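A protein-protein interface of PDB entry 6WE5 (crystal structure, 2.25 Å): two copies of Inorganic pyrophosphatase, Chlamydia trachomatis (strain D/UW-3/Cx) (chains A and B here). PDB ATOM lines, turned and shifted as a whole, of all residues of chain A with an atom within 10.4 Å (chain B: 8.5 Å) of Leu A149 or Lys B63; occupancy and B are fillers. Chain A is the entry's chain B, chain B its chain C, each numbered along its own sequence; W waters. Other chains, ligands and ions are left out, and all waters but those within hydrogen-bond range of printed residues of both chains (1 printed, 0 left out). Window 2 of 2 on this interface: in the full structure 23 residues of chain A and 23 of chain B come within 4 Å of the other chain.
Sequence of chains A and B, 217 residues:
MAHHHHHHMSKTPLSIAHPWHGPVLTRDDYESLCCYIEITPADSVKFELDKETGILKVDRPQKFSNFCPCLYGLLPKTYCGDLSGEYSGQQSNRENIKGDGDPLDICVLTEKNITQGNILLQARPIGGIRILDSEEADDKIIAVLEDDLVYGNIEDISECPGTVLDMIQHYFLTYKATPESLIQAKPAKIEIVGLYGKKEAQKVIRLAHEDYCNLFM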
ATOM      1  N   LEU A 109     -10.405  -1.341   0.028  1.00  0.00           N
ATOM      2  CA  LEU A 109      -9.425  -0.749   0.928  1.00  0.00           C
ATOM      3  C   LEU A 109      -9.680   0.749   1.063  1.00  0.00           C
ATOM      4  O   LEU A 109      -9.830   1.455   0.056  1.00  0.00           O
ATOM      5  CB  LEU A 109      -8.009  -0.991   0.405  1.00  0.00           C
ATOM      6  CG  LEU A 109      -7.624  -2.442   0.113  1.00  0.00           C
ATOM      7  CD1 LEU A 109      -6.204  -2.513  -0.392  1.00  0.00           C
ATOM      8  CD2 LEU A 109      -7.794  -3.296   1.369  1.00  0.00           C
ATOM      9  N   THR A 110      -9.726   1.227   2.306  1.00  0.00           N
ATOM     10  CA  THR A 110      -9.862   2.651   2.570  1.00  0.00           C
ATOM     11  C   THR A 110      -9.175   2.993   3.886  1.00  0.00           C
ATOM     12  O   THR A 110      -9.133   2.186   4.819  1.00  0.00           O
ATOM     13  CB  THR A 110     -11.333   3.090   2.608  1.00  0.00           C
ATOM     14  OG1 THR A 110     -11.418   4.476   2.964  1.00  0.00           O
ATOM     15  CG2 THR A 110     -12.118   2.259   3.615  1.00  0.00           C
ATOM     16  N   GLU A 111      -8.624   4.205   3.939  1.00  0.00           N
ATOM     17  CA  GLU A 111      -8.064   4.750   5.168  1.00  0.00           C
ATOM     18  C   GLU A 111      -9.144   5.256   6.126  1.00  0.00           C
ATOM     19  O   GLU A 111      -8.902   5.332   7.335  1.00  0.00           O
ATOM     20  CB  GLU A 111      -7.071   5.867   4.796  1.00  0.00           C
ATOM     21  CG  GLU A 111      -6.847   6.972   5.826  1.00  0.00           C
ATOM     22  CD  GLU A 111      -7.694   8.200   5.569  1.00  0.00           C
ATOM     23  OE1 GLU A 111      -8.267   8.317   4.464  1.00  0.00           O
ATOM     24  OE2 GLU A 111      -7.788   9.051   6.479  1.00  0.00           O
ATOM     25  N   LYS A 112     -10.332   5.572   5.621  1.00  0.00           N
ATOM     26  CA  LYS A 112     -11.395   6.136   6.439  1.00  0.00           C
ATOM     27  C   LYS A 112     -12.126   5.055   7.237  1.00  0.00           C
ATOM     28  O   LYS A 112     -12.139   3.874   6.878  1.00  0.00           O
ATOM     29  CB  LYS A 112     -12.406   6.876   5.561  1.00  0.00           C
ATOM     30  CG  LYS A 112     -11.936   8.221   5.021  1.00  0.00           C
ATOM     31  CD  LYS A 112     -11.405   9.119   6.121  1.00  0.00           C
ATOM     32  CE  LYS A 112     -11.111  10.513   5.574  1.00  0.00           C
ATOM     33  NZ  LYS A 112      -9.966  11.177   6.258  1.00  0.00           N
ATOM     34  N   ASN A 113     -12.766   5.487   8.320  1.00  0.00           N
ATOM     35  CA  ASN A 113     -13.628   4.622   9.120  1.00  0.00           C
ATOM     36  C   ASN A 113     -15.064   4.709   8.623  1.00  0.00           C
ATOM     37  O   ASN A 113     -15.708   5.761   8.726  1.00  0.00           O
ATOM     38  CB  ASN A 113     -13.569   4.981  10.600  1.00  0.00           C
ATOM     39  CG  ASN A 113     -13.080   3.846  11.436  1.00  0.00           C
ATOM     40  OD1 ASN A 113     -11.900   3.508  11.428  1.00  0.00           O
ATOM     41  ND2 ASN A 113     -14.003   3.216  12.155  1.00  0.00           N
ATOM     42  N   VAL A 144      -9.695  -0.419  -4.316  1.00  0.00           N
ATOM     43  CA  VAL A 144      -9.429   0.724  -3.458  1.00  0.00           C
ATOM     44  C   VAL A 144     -10.587   1.698  -3.600  1.00  0.00           C
ATOM     45  O   VAL A 144     -11.148   1.860  -4.690  1.00  0.00           O
ATOM     46  CB  VAL A 144      -8.081   1.394  -3.794  1.00  0.00           C
ATOM     47  CG1 VAL A 144      -6.947   0.403  -3.610  1.00  0.00           C
ATOM     48  CG2 VAL A 144      -8.074   1.967  -5.210  1.00  0.00           C
ATOM     49  N   LEU A 145     -10.996   2.282  -2.477  1.00  0.00           N
ATOM     50  CA  LEU A 145     -12.046   3.287  -2.509  1.00  0.00           C
ATOM     51  C   LEU A 145     -11.598   4.458  -3.376  1.00  0.00           C
ATOM     52  O   LEU A 145     -10.466   4.934  -3.252  1.00  0.00           O
ATOM     53  CB  LEU A 145     -12.362   3.757  -1.090  1.00  0.00           C
ATOM     54  CG  LEU A 145     -13.333   4.931  -0.952  1.00  0.00           C
ATOM     55  CD1 LEU A 145     -14.731   4.522  -1.389  1.00  0.00           C
ATOM     56  CD2 LEU A 145     -13.329   5.480   0.475  1.00  0.00           C
ATOM     57  N   GLU A 146     -12.473   4.892  -4.285  1.00  0.00           N
ATOM     58  CA  GLU A 146     -12.144   6.010  -5.163  1.00  0.00           C
ATOM     59  C   GLU A 146     -11.876   7.264  -4.344  1.00  0.00           C
ATOM     60  O   GLU A 146     -12.611   7.570  -3.398  1.00  0.00           O
ATOM     61  CB  GLU A 146     -13.272   6.266  -6.164  1.00  0.00           C
ATOM     62  CG  GLU A 146     -12.845   7.090  -7.383  1.00  0.00           C
ATOM     63  CD  GLU A 146     -13.696   6.815  -8.620  1.00  0.00           C
ATOM     64  OE1 GLU A 146     -13.149   6.326  -9.635  1.00  0.00           O
ATOM     65  OE2 GLU A 146     -14.914   7.093  -8.580  1.00  0.00           O
ATOM     66  N   ASP A 147     -10.803   7.972  -4.698  1.00  0.00           N
ATOM     67  CA  ASP A 147     -10.389   9.211  -4.040  1.00  0.00           C
ATOM     68  C   ASP A 147      -9.999   8.996  -2.583  1.00  0.00           C
ATOM     69  O   ASP A 147      -9.958   9.950  -1.802  1.00  0.00           O
ATOM     70  CB  ASP A 147     -11.480  10.288  -4.129  1.00  0.00           C
ATOM     71  CG  ASP A 147     -11.809  10.672  -5.560  1.00  0.00           C
ATOM     72  OD1 ASP A 147     -10.911  10.587  -6.425  1.00  0.00           O
ATOM     73  OD2 ASP A 147     -12.971  11.050  -5.819  1.00  0.00           O
ATOM     74  N   ASP A 148      -9.687   7.765  -2.190  1.00  0.00           N
ATOM     75  CA  ASP A 148      -9.208   7.546  -0.836  1.00  0.00           C
ATOM     76  C   ASP A 148      -7.864   8.237  -0.650  1.00  0.00           C
ATOM     77  O   ASP A 148      -7.024   8.242  -1.552  1.00  0.00           O
ATOM     78  CB  ASP A 148      -9.088   6.054  -0.542  1.00  0.00           C
ATOM     79  CG  ASP A 148      -8.660   5.784   0.880  1.00  0.00           C
ATOM     80  OD1 ASP A 148      -9.538   5.766   1.768  1.00  0.00           O
ATOM     81  OD2 ASP A 148      -7.451   5.585   1.112  1.00  0.00           O
ATOM     82  N   LEU A 149      -7.664   8.834   0.526  1.00  0.00           N
ATOM     83  CA  LEU A 149      -6.485   9.667   0.721  1.00  0.00           C
ATOM     84  C   LEU A 149      -5.198   8.858   0.739  1.00  0.00           C
ATOM     85  O   LEU A 149      -4.123   9.428   0.530  1.00  0.00           O
ATOM     86  CB  LEU A 149      -6.598  10.471   2.019  1.00  0.00           C
ATOM     87  CG  LEU A 149      -7.793  11.424   2.140  1.00  0.00           C
ATOM     88  CD1 LEU A 149      -7.653  12.349   3.364  1.00  0.00           C
ATOM     89  CD2 LEU A 149      -7.962  12.228   0.867  1.00  0.00           C
ATOM     90  N   VAL A 150      -5.274   7.548   0.964  1.00  0.00           N
ATOM     91  CA  VAL A 150      -4.094   6.698   1.075  1.00  0.00           C
ATOM     92  C   VAL A 150      -3.987   5.729  -0.099  1.00  0.00           C
ATOM     93  O   VAL A 150      -2.965   5.682  -0.784  1.00  0.00           O
ATOM     94  CB  VAL A 150      -4.083   5.944   2.423  1.00  0.00           C
ATOM     95  CG1 VAL A 150      -3.059   4.829   2.401  1.00  0.00           C
ATOM     96  CG2 VAL A 150      -3.788   6.915   3.567  1.00  0.00           C
ATOM     97  N   TYR A 151      -5.044   4.966  -0.361  1.00  0.00           N
ATOM     98  CA  TYR A 151      -5.023   3.928  -1.384  1.00  0.00           C
ATOM     99  C   TYR A 151      -5.527   4.412  -2.737  1.00  0.00           C
ATOM    100  O   TYR A 151      -5.529   3.631  -3.695  1.00  0.00           O
ATOM    101  CB  TYR A 151      -5.873   2.730  -0.940  1.00  0.00           C
ATOM    102  CG  TYR A 151      -5.503   2.149   0.406  1.00  0.00           C
ATOM    103  CD1 TYR A 151      -4.520   1.173   0.521  1.00  0.00           C
ATOM    104  CD2 TYR A 151      -6.169   2.543   1.557  1.00  0.00           C
ATOM    105  CE1 TYR A 151      -4.188   0.631   1.755  1.00  0.00           C
ATOM    106  CE2 TYR A 151      -5.845   2.006   2.793  1.00  0.00           C
ATOM    107  CZ  TYR A 151      -4.855   1.053   2.884  1.00  0.00           C
ATOM    108  OH  TYR A 151      -4.531   0.517   4.108  1.00  0.00           O
ATOM    109  N   GLY A 152      -5.943   5.678  -2.839  1.00  0.00           N
ATOM    110  CA  GLY A 152      -6.636   6.137  -4.030  1.00  0.00           C
ATOM    111  C   GLY A 152      -5.833   6.014  -5.310  1.00  0.00           C
ATOM    112  O   GLY A 152      -6.400   5.753  -6.375  1.00  0.00           O
ATOM    113  N   ASN A 153      -4.513   6.180  -5.234  1.00  0.00           N
ATOM    114  CA  ASN A 153      -3.684   6.166  -6.434  1.00  0.00           C
ATOM    115  C   ASN A 153      -3.103   4.797  -6.756  1.00  0.00           C
ATOM    116  O   ASN A 153      -2.386   4.665  -7.753  1.00  0.00           O
ATOM    117  CB  ASN A 153      -2.532   7.166  -6.299  1.00  0.00           C
ATOM    118  CG  ASN A 153      -3.006   8.596  -6.218  1.00  0.00           C
ATOM    119  OD1 ASN A 153      -3.904   9.011  -6.949  1.00  0.00           O
ATOM    120  ND2 ASN A 153      -2.390   9.368  -5.330  1.00  0.00           N
ATOM    121  N   ILE A 154      -3.414   3.774  -5.966  1.00  0.00           N
ATOM    122  CA  ILE A 154      -2.912   2.438  -6.250  1.00  0.00           C
ATOM    123  C   ILE A 154      -3.634   1.877  -7.468  1.00  0.00           C
ATOM    124  O   ILE A 154      -4.871   1.876  -7.536  1.00  0.00           O
ATOM    125  CB  ILE A 154      -3.075   1.534  -5.022  1.00  0.00           C
ATOM    126  CG1 ILE A 154      -2.206   2.073  -3.882  1.00  0.00           C
ATOM    127  CG2 ILE A 154      -2.724   0.098  -5.379  1.00  0.00           C
ATOM    128  CD1 ILE A 154      -2.183   1.202  -2.648  1.00  0.00           C
ATOM    129  N   SER B  44     -16.941   9.868   8.519  1.00  0.00           N
ATOM    130  CA  SER B  44     -15.678  10.366   7.993  1.00  0.00           C
ATOM    131  C   SER B  44     -15.689  10.479   6.481  1.00  0.00           C
ATOM    132  O   SER B  44     -14.680  10.883   5.892  1.00  0.00           O
ATOM    133  CB  SER B  44     -14.518   9.469   8.432  1.00  0.00           C
ATOM    134  OG  SER B  44     -14.532   9.291   9.830  1.00  0.00           O
ATOM    135  N   VAL B  45     -16.790  10.096   5.840  1.00  0.00           N
ATOM    136  CA  VAL B  45     -16.977  10.270   4.409  1.00  0.00           C
ATOM    137  C   VAL B  45     -18.289  11.007   4.209  1.00  0.00           C
ATOM    138  O   VAL B  45     -19.142  11.061   5.097  1.00  0.00           O
ATOM    139  CB  VAL B  45     -16.992   8.928   3.638  1.00  0.00           C
ATOM    140  CG1 VAL B  45     -15.707   8.141   3.893  1.00  0.00           C
ATOM    141  CG2 VAL B  45     -18.209   8.113   4.024  1.00  0.00           C
ATOM    142  N   LYS B  46     -18.428  11.591   3.026  1.00  0.00           N
ATOM    143  CA  LYS B  46     -19.650  12.278   2.631  1.00  0.00           C
ATOM    144  C   LYS B  46     -20.552  11.287   1.897  1.00  0.00           C
ATOM    145  O   LYS B  46     -20.203  10.799   0.817  1.00  0.00           O
ATOM    146  CB  LYS B  46     -19.315  13.496   1.770  1.00  0.00           C
ATOM    147  CG  LYS B  46     -18.537  14.564   2.544  1.00  0.00           C
ATOM    148  CD  LYS B  46     -18.509  15.920   1.848  1.00  0.00           C
ATOM    149  CE  LYS B  46     -17.540  15.938   0.675  1.00  0.00           C
ATOM    150  NZ  LYS B  46     -17.831  17.044  -0.285  1.00  0.00           N
ATOM    151  N   ARG B  60     -17.716  10.830  -1.511  1.00  0.00           N
ATOM    152  CA  ARG B  60     -16.272  11.009  -1.437  1.00  0.00           C
ATOM    153  C   ARG B  60     -15.869  10.991   0.027  1.00  0.00           C
ATOM    154  O   ARG B  60     -16.683  11.334   0.891  1.00  0.00           O
ATOM    155  CB  ARG B  60     -15.840  12.332  -2.087  1.00  0.00           C
ATOM    156  N   PRO B  61     -14.645  10.582   0.344  1.00  0.00           N
ATOM    157  CA  PRO B  61     -14.166  10.736   1.723  1.00  0.00           C
ATOM    158  C   PRO B  61     -13.989  12.210   2.049  1.00  0.00           C
ATOM    159  O   PRO B  61     -13.789  13.037   1.157  1.00  0.00           O
ATOM    160  CB  PRO B  61     -12.826   9.991   1.723  1.00  0.00           C
ATOM    161  CG  PRO B  61     -12.389   9.991   0.289  1.00  0.00           C
ATOM    162  CD  PRO B  61     -13.634   9.979  -0.544  1.00  0.00           C
ATOM    163  N   GLN B  62     -14.084  12.545   3.336  1.00  0.00           N
ATOM    164  CA  GLN B  62     -13.745  13.902   3.759  1.00  0.00           C
ATOM    165  C   GLN B  62     -12.322  14.214   3.318  1.00  0.00           C
ATOM    166  O   GLN B  62     -11.399  13.427   3.557  1.00  0.00           O
ATOM    167  CB  GLN B  62     -13.875  14.065   5.283  1.00  0.00           C
ATOM    168  CG  GLN B  62     -15.310  14.104   5.817  1.00  0.00           C
ATOM    169  CD  GLN B  62     -16.012  15.436   5.562  1.00  0.00           C
ATOM    170  OE1 GLN B  62     -15.406  16.394   5.073  1.00  0.00           O
ATOM    171  NE2 GLN B  62     -17.304  15.491   5.877  1.00  0.00           N
ATOM    172  N   LYS B  63     -12.148  15.338   2.625  1.00  0.00           N
ATOM    173  CA  LYS B  63     -10.827  15.636   2.091  1.00  0.00           C
ATOM    174  C   LYS B  63      -9.873  16.136   3.165  1.00  0.00           C
ATOM    175  O   LYS B  63      -8.658  15.946   3.043  1.00  0.00           O
ATOM    176  CB  LYS B  63     -10.914  16.659   0.956  1.00  0.00           C
ATOM    177  CG  LYS B  63      -9.645  16.697   0.116  1.00  0.00           C
ATOM    178  CD  LYS B  63      -9.735  17.664  -1.040  1.00  0.00           C
ATOM    179  CE  LYS B  63      -8.387  17.786  -1.738  1.00  0.00           C
ATOM    180  NZ  LYS B  63      -8.421  18.730  -2.892  1.00  0.00           N
ATOM    181  N   PHE B  64     -10.382  16.798   4.198  1.00  0.00           N
ATOM    182  CA  PHE B  64      -9.487  17.416   5.168  1.00  0.00           C
ATOM    183  C   PHE B  64      -9.879  17.040   6.591  1.00  0.00           C
ATOM    184  O   PHE B  64     -10.146  15.866   6.865  1.00  0.00           O
ATOM    185  CB  PHE B  64      -9.474  18.932   4.970  1.00  0.00           C
ATOM    186  CG  PHE B  64      -9.109  19.344   3.580  1.00  0.00           C
ATOM    187  CD1 PHE B  64      -7.853  19.067   3.068  1.00  0.00           C
ATOM    188  CD2 PHE B  64     -10.033  19.989   2.770  1.00  0.00           C
ATOM    189  CE1 PHE B  64      -7.519  19.435   1.778  1.00  0.00           C
ATOM    190  CE2 PHE B  64      -9.707  20.365   1.483  1.00  0.00           C
ATOM    191  CZ  PHE B  64      -8.447  20.091   0.987  1.00  0.00           C
ATOM    192  N   SER B  65      -9.943  18.018   7.503  1.00  0.00           N
ATOM    193  CA  SER B  65     -10.081  17.725   8.925  1.00  0.00           C
ATOM    194  C   SER B  65     -11.477  18.028   9.464  1.00  0.00           C
ATOM    195  O   SER B  65     -11.628  18.338  10.646  1.00  0.00           O
ATOM    196  CB  SER B  65      -9.009  18.472   9.729  1.00  0.00           C
ATOM    197  OG  SER B  65      -9.186  19.872   9.698  1.00  0.00           O
ATOM    198  N   ASN B  66     -12.509  17.871   8.636  1.00  0.00           N
ATOM    199  CA  ASN B  66     -13.870  18.227   9.010  1.00  0.00           C
ATOM    200  C   ASN B  66     -14.723  16.999   9.306  1.00  0.00           C
ATOM    201  O   ASN B  66     -14.571  15.940   8.691  1.00  0.00           O
ATOM    202  CB  ASN B  66     -14.577  19.025   7.899  1.00  0.00           C
ATOM    203  CG  ASN B  66     -13.854  20.295   7.541  1.00  0.00           C
ATOM    204  OD1 ASN B  66     -13.036  20.316   6.626  1.00  0.00           O
ATOM    205  ND2 ASN B  66     -14.131  21.361   8.278  1.00  0.00           N
ATOM    206  N   TYR B 171     -18.165  24.692   8.565  1.00  0.00           N
ATOM    207  CA  TYR B 171     -18.058  23.447   7.811  1.00  0.00           C
ATOM    208  C   TYR B 171     -18.050  23.718   6.311  1.00  0.00           C
ATOM    209  O   TYR B 171     -17.123  23.311   5.600  1.00  0.00           O
ATOM    210  CB  TYR B 171     -19.194  22.499   8.190  1.00  0.00           C
ATOM    211  CG  TYR B 171     -19.225  21.209   7.390  1.00  0.00           C
ATOM    212  CD1 TYR B 171     -18.276  20.215   7.598  1.00  0.00           C
ATOM    213  CD2 TYR B 171     -20.210  20.983   6.427  1.00  0.00           C
ATOM    214  CE1 TYR B 171     -18.300  19.023   6.874  1.00  0.00           C
ATOM    215  CE2 TYR B 171     -20.249  19.795   5.698  1.00  0.00           C
ATOM    216  CZ  TYR B 171     -19.288  18.821   5.924  1.00  0.00           C
ATOM    217  OH  TYR B 171     -19.315  17.645   5.205  1.00  0.00           O
ATOM    218  N   THR B 174     -14.894  25.521   4.983  1.00  0.00           N
ATOM    219  CA  THR B 174     -13.577  24.900   5.041  1.00  0.00           C
ATOM    220  C   THR B 174     -13.513  23.478   4.503  1.00  0.00           C
ATOM    221  O   THR B 174     -12.408  23.019   4.191  1.00  0.00           O
ATOM    222  CB  THR B 174     -13.024  24.877   6.486  1.00  0.00           C
ATOM    223  OG1 THR B 174     -13.893  24.119   7.344  1.00  0.00           O
ATOM    224  CG2 THR B 174     -12.874  26.283   7.036  1.00  0.00           C
ATOM    225  N   TYR B 175     -14.640  22.771   4.364  1.00  0.00           N
ATOM    226  CA  TYR B 175     -14.524  21.342   4.066  1.00  0.00           C
ATOM    227  C   TYR B 175     -13.970  21.067   2.674  1.00  0.00           C
ATOM    228  O   TYR B 175     -13.626  19.916   2.389  1.00  0.00           O
ATOM    229  CB  TYR B 175     -15.862  20.609   4.272  1.00  0.00           C
ATOM    230  CG  TYR B 175     -16.905  20.745   3.176  1.00  0.00           C
ATOM    231  CD1 TYR B 175     -17.216  21.980   2.610  1.00  0.00           C
ATOM    232  CD2 TYR B 175     -17.602  19.629   2.731  1.00  0.00           C
ATOM    233  CE1 TYR B 175     -18.183  22.086   1.612  1.00  0.00           C
ATOM    234  CE2 TYR B 175     -18.564  19.726   1.744  1.00  0.00           C
ATOM    235  CZ  TYR B 175     -18.851  20.949   1.189  1.00  0.00           C
ATOM    236  OH  TYR B 175     -19.811  21.022   0.210  1.00  0.00           O
ATOM    237  N   LYS B 176     -13.858  22.083   1.816  1.00  0.00           N
ATOM    238  CA  LYS B 176     -13.235  21.934   0.505  1.00  0.00           C
ATOM    239  C   LYS B 176     -12.078  22.908   0.296  1.00  0.00           C
ATOM    240  O   LYS B 176     -11.574  23.022  -0.827  1.00  0.00           O
ATOM    241  CB  LYS B 176     -14.278  22.106  -0.610  1.00  0.00           C
ATOM    242  N   ALA B 177     -11.618  23.575   1.351  1.00  0.00           N
ATOM    243  CA  ALA B 177     -10.591  24.605   1.242  1.00  0.00           C
ATOM    244  C   ALA B 177      -9.206  23.979   1.345  1.00  0.00           C
ATOM    245  O   ALA B 177      -8.862  23.388   2.374  1.00  0.00           O
ATOM    246  CB  ALA B 177     -10.775  25.659   2.333  1.00  0.00           C
ATOM    247  N   THR B 178      -8.406  24.129   0.291  1.00  0.00           N
ATOM    248  CA  THR B 178      -7.064  23.572   0.304  1.00  0.00           C
ATOM    249  C   THR B 178      -6.167  24.379   1.244  1.00  0.00           C
ATOM    250  O   THR B 178      -6.415  25.565   1.481  1.00  0.00           O
ATOM    251  CB  THR B 178      -6.474  23.574  -1.105  1.00  0.00           C
ATOM    252  OG1 THR B 178      -6.241  24.924  -1.519  1.00  0.00           O
ATOM    253  CG2 THR B 178      -7.436  22.911  -2.085  1.00  0.00           C
ATOM    254  N   PRO B 179      -5.120  23.757   1.800  1.00  0.00           N
ATOM    255  CA  PRO B 179      -4.171  24.534   2.620  1.00  0.00           C
ATOM    256  C   PRO B 179      -3.573  25.718   1.880  1.00  0.00           C
ATOM    257  O   PRO B 179      -3.478  26.813   2.449  1.00  0.00           O
ATOM    258  CB  PRO B 179      -3.117  23.490   3.002  1.00  0.00           C
ATOM    259  CG  PRO B 179      -3.872  22.214   3.016  1.00  0.00           C
ATOM    260  CD  PRO B 179      -4.814  22.318   1.840  1.00  0.00           C
HETATM  261  O   HOH W   1     -17.666   7.153   7.802  1.00  0.00           O
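The side-chain hydroxyl (OG1) of Thr A110 lies within hydrogen-bond range of the backbone NH (N) of Lys A112. OE2 of Glu A111 is in salt-bridge range of NZ of Lys A112, 3.1 Å away. The backbone carbonyl oxygen of Ser B44 is in hydrogen-bond range of the backbone NH of Gln B62, 3.1 Å away. The side-chain amide nitrogen (NE2) of Gln B62 lies within hydrogen-bond range of the side-chain hydroxyl (OH) of Tyr B171 (3.0 Å).
Lys A112 touches Ser B44. CB of Lys A112 touches CG1 of Val B45, 3.9 Å away. CG of Lys A112 touches CB of Pro B61, 3.8 Å away. Gln B62 touches Lys A112. Asn A113 touches Ser B44. O of Glu A146 touches CD of Pro B61 (3.9 Å). CG of Pro B61 touches O of Asp A147, at 3.2 Å. CD1 of Leu A149 touches O of Gln B62 (3.9 Å). CD1 of Leu A149 touches O of Lys B63, 3.7 Å away.
Of chain B, only Gln B62 (3.9 Å) and Lys B63 (3.7 Å) come within 4 Å of Leu A149. Printed residues of chain A within 4 Å of Lys B63: Leu A149. No residue of chain B comes within 4 Å of Asp A148. Pro B61 touches three residues of chain A. No residue of chain A comes within 4 Å of Phe B64. Of the printed residues of chain B, Asp A147 touches Pro B61 (3.2 Å). Of the printed residues of chain B, Glu A146 touches Pro B61. Val A150 touches none of the printed residues of chain B. The nearest residue of chain B that does not touch Leu A149 is Pro B61 (4.9 Å). The nearest residue of chain A that does not touch Lys B63 is Lys A112 (5.7 Å). The nearest printed residue of chain B that does not touch Lys A112 is Phe B64 (4.7 Å).
Of the 17 printed residues of chain B, 5 touch a printed residue of chain A. Printed residues of chain B that touch a printed residue of chain A: Ser B44, Val B45, Pro B61, Gln B62 and Lys B63. Printed residues of chain A that touch a printed residue of chain B: Lys A112, Asn A113, Glu A146, Asp A147 and Leu A149. Along chain A the printed residues that touch a printed residue of chain B span positions 112 to 149. Among the printed residues, 9 pairs touch across the chains. Among the printed residues, no Asp or Glu carboxylate lies within 4 Å of a Lys or Arg side-chain nitrogen of the other chain.
No position is printed for both chains. Of the 9 pairs that touch across the chains among the printed residues, none has its exchanged pair printed and touching as well.
Water W1 lies within hydrogen-bond range of O of Asn A113 (2.6 Å) and N of Ser B44 (2.9 Å).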
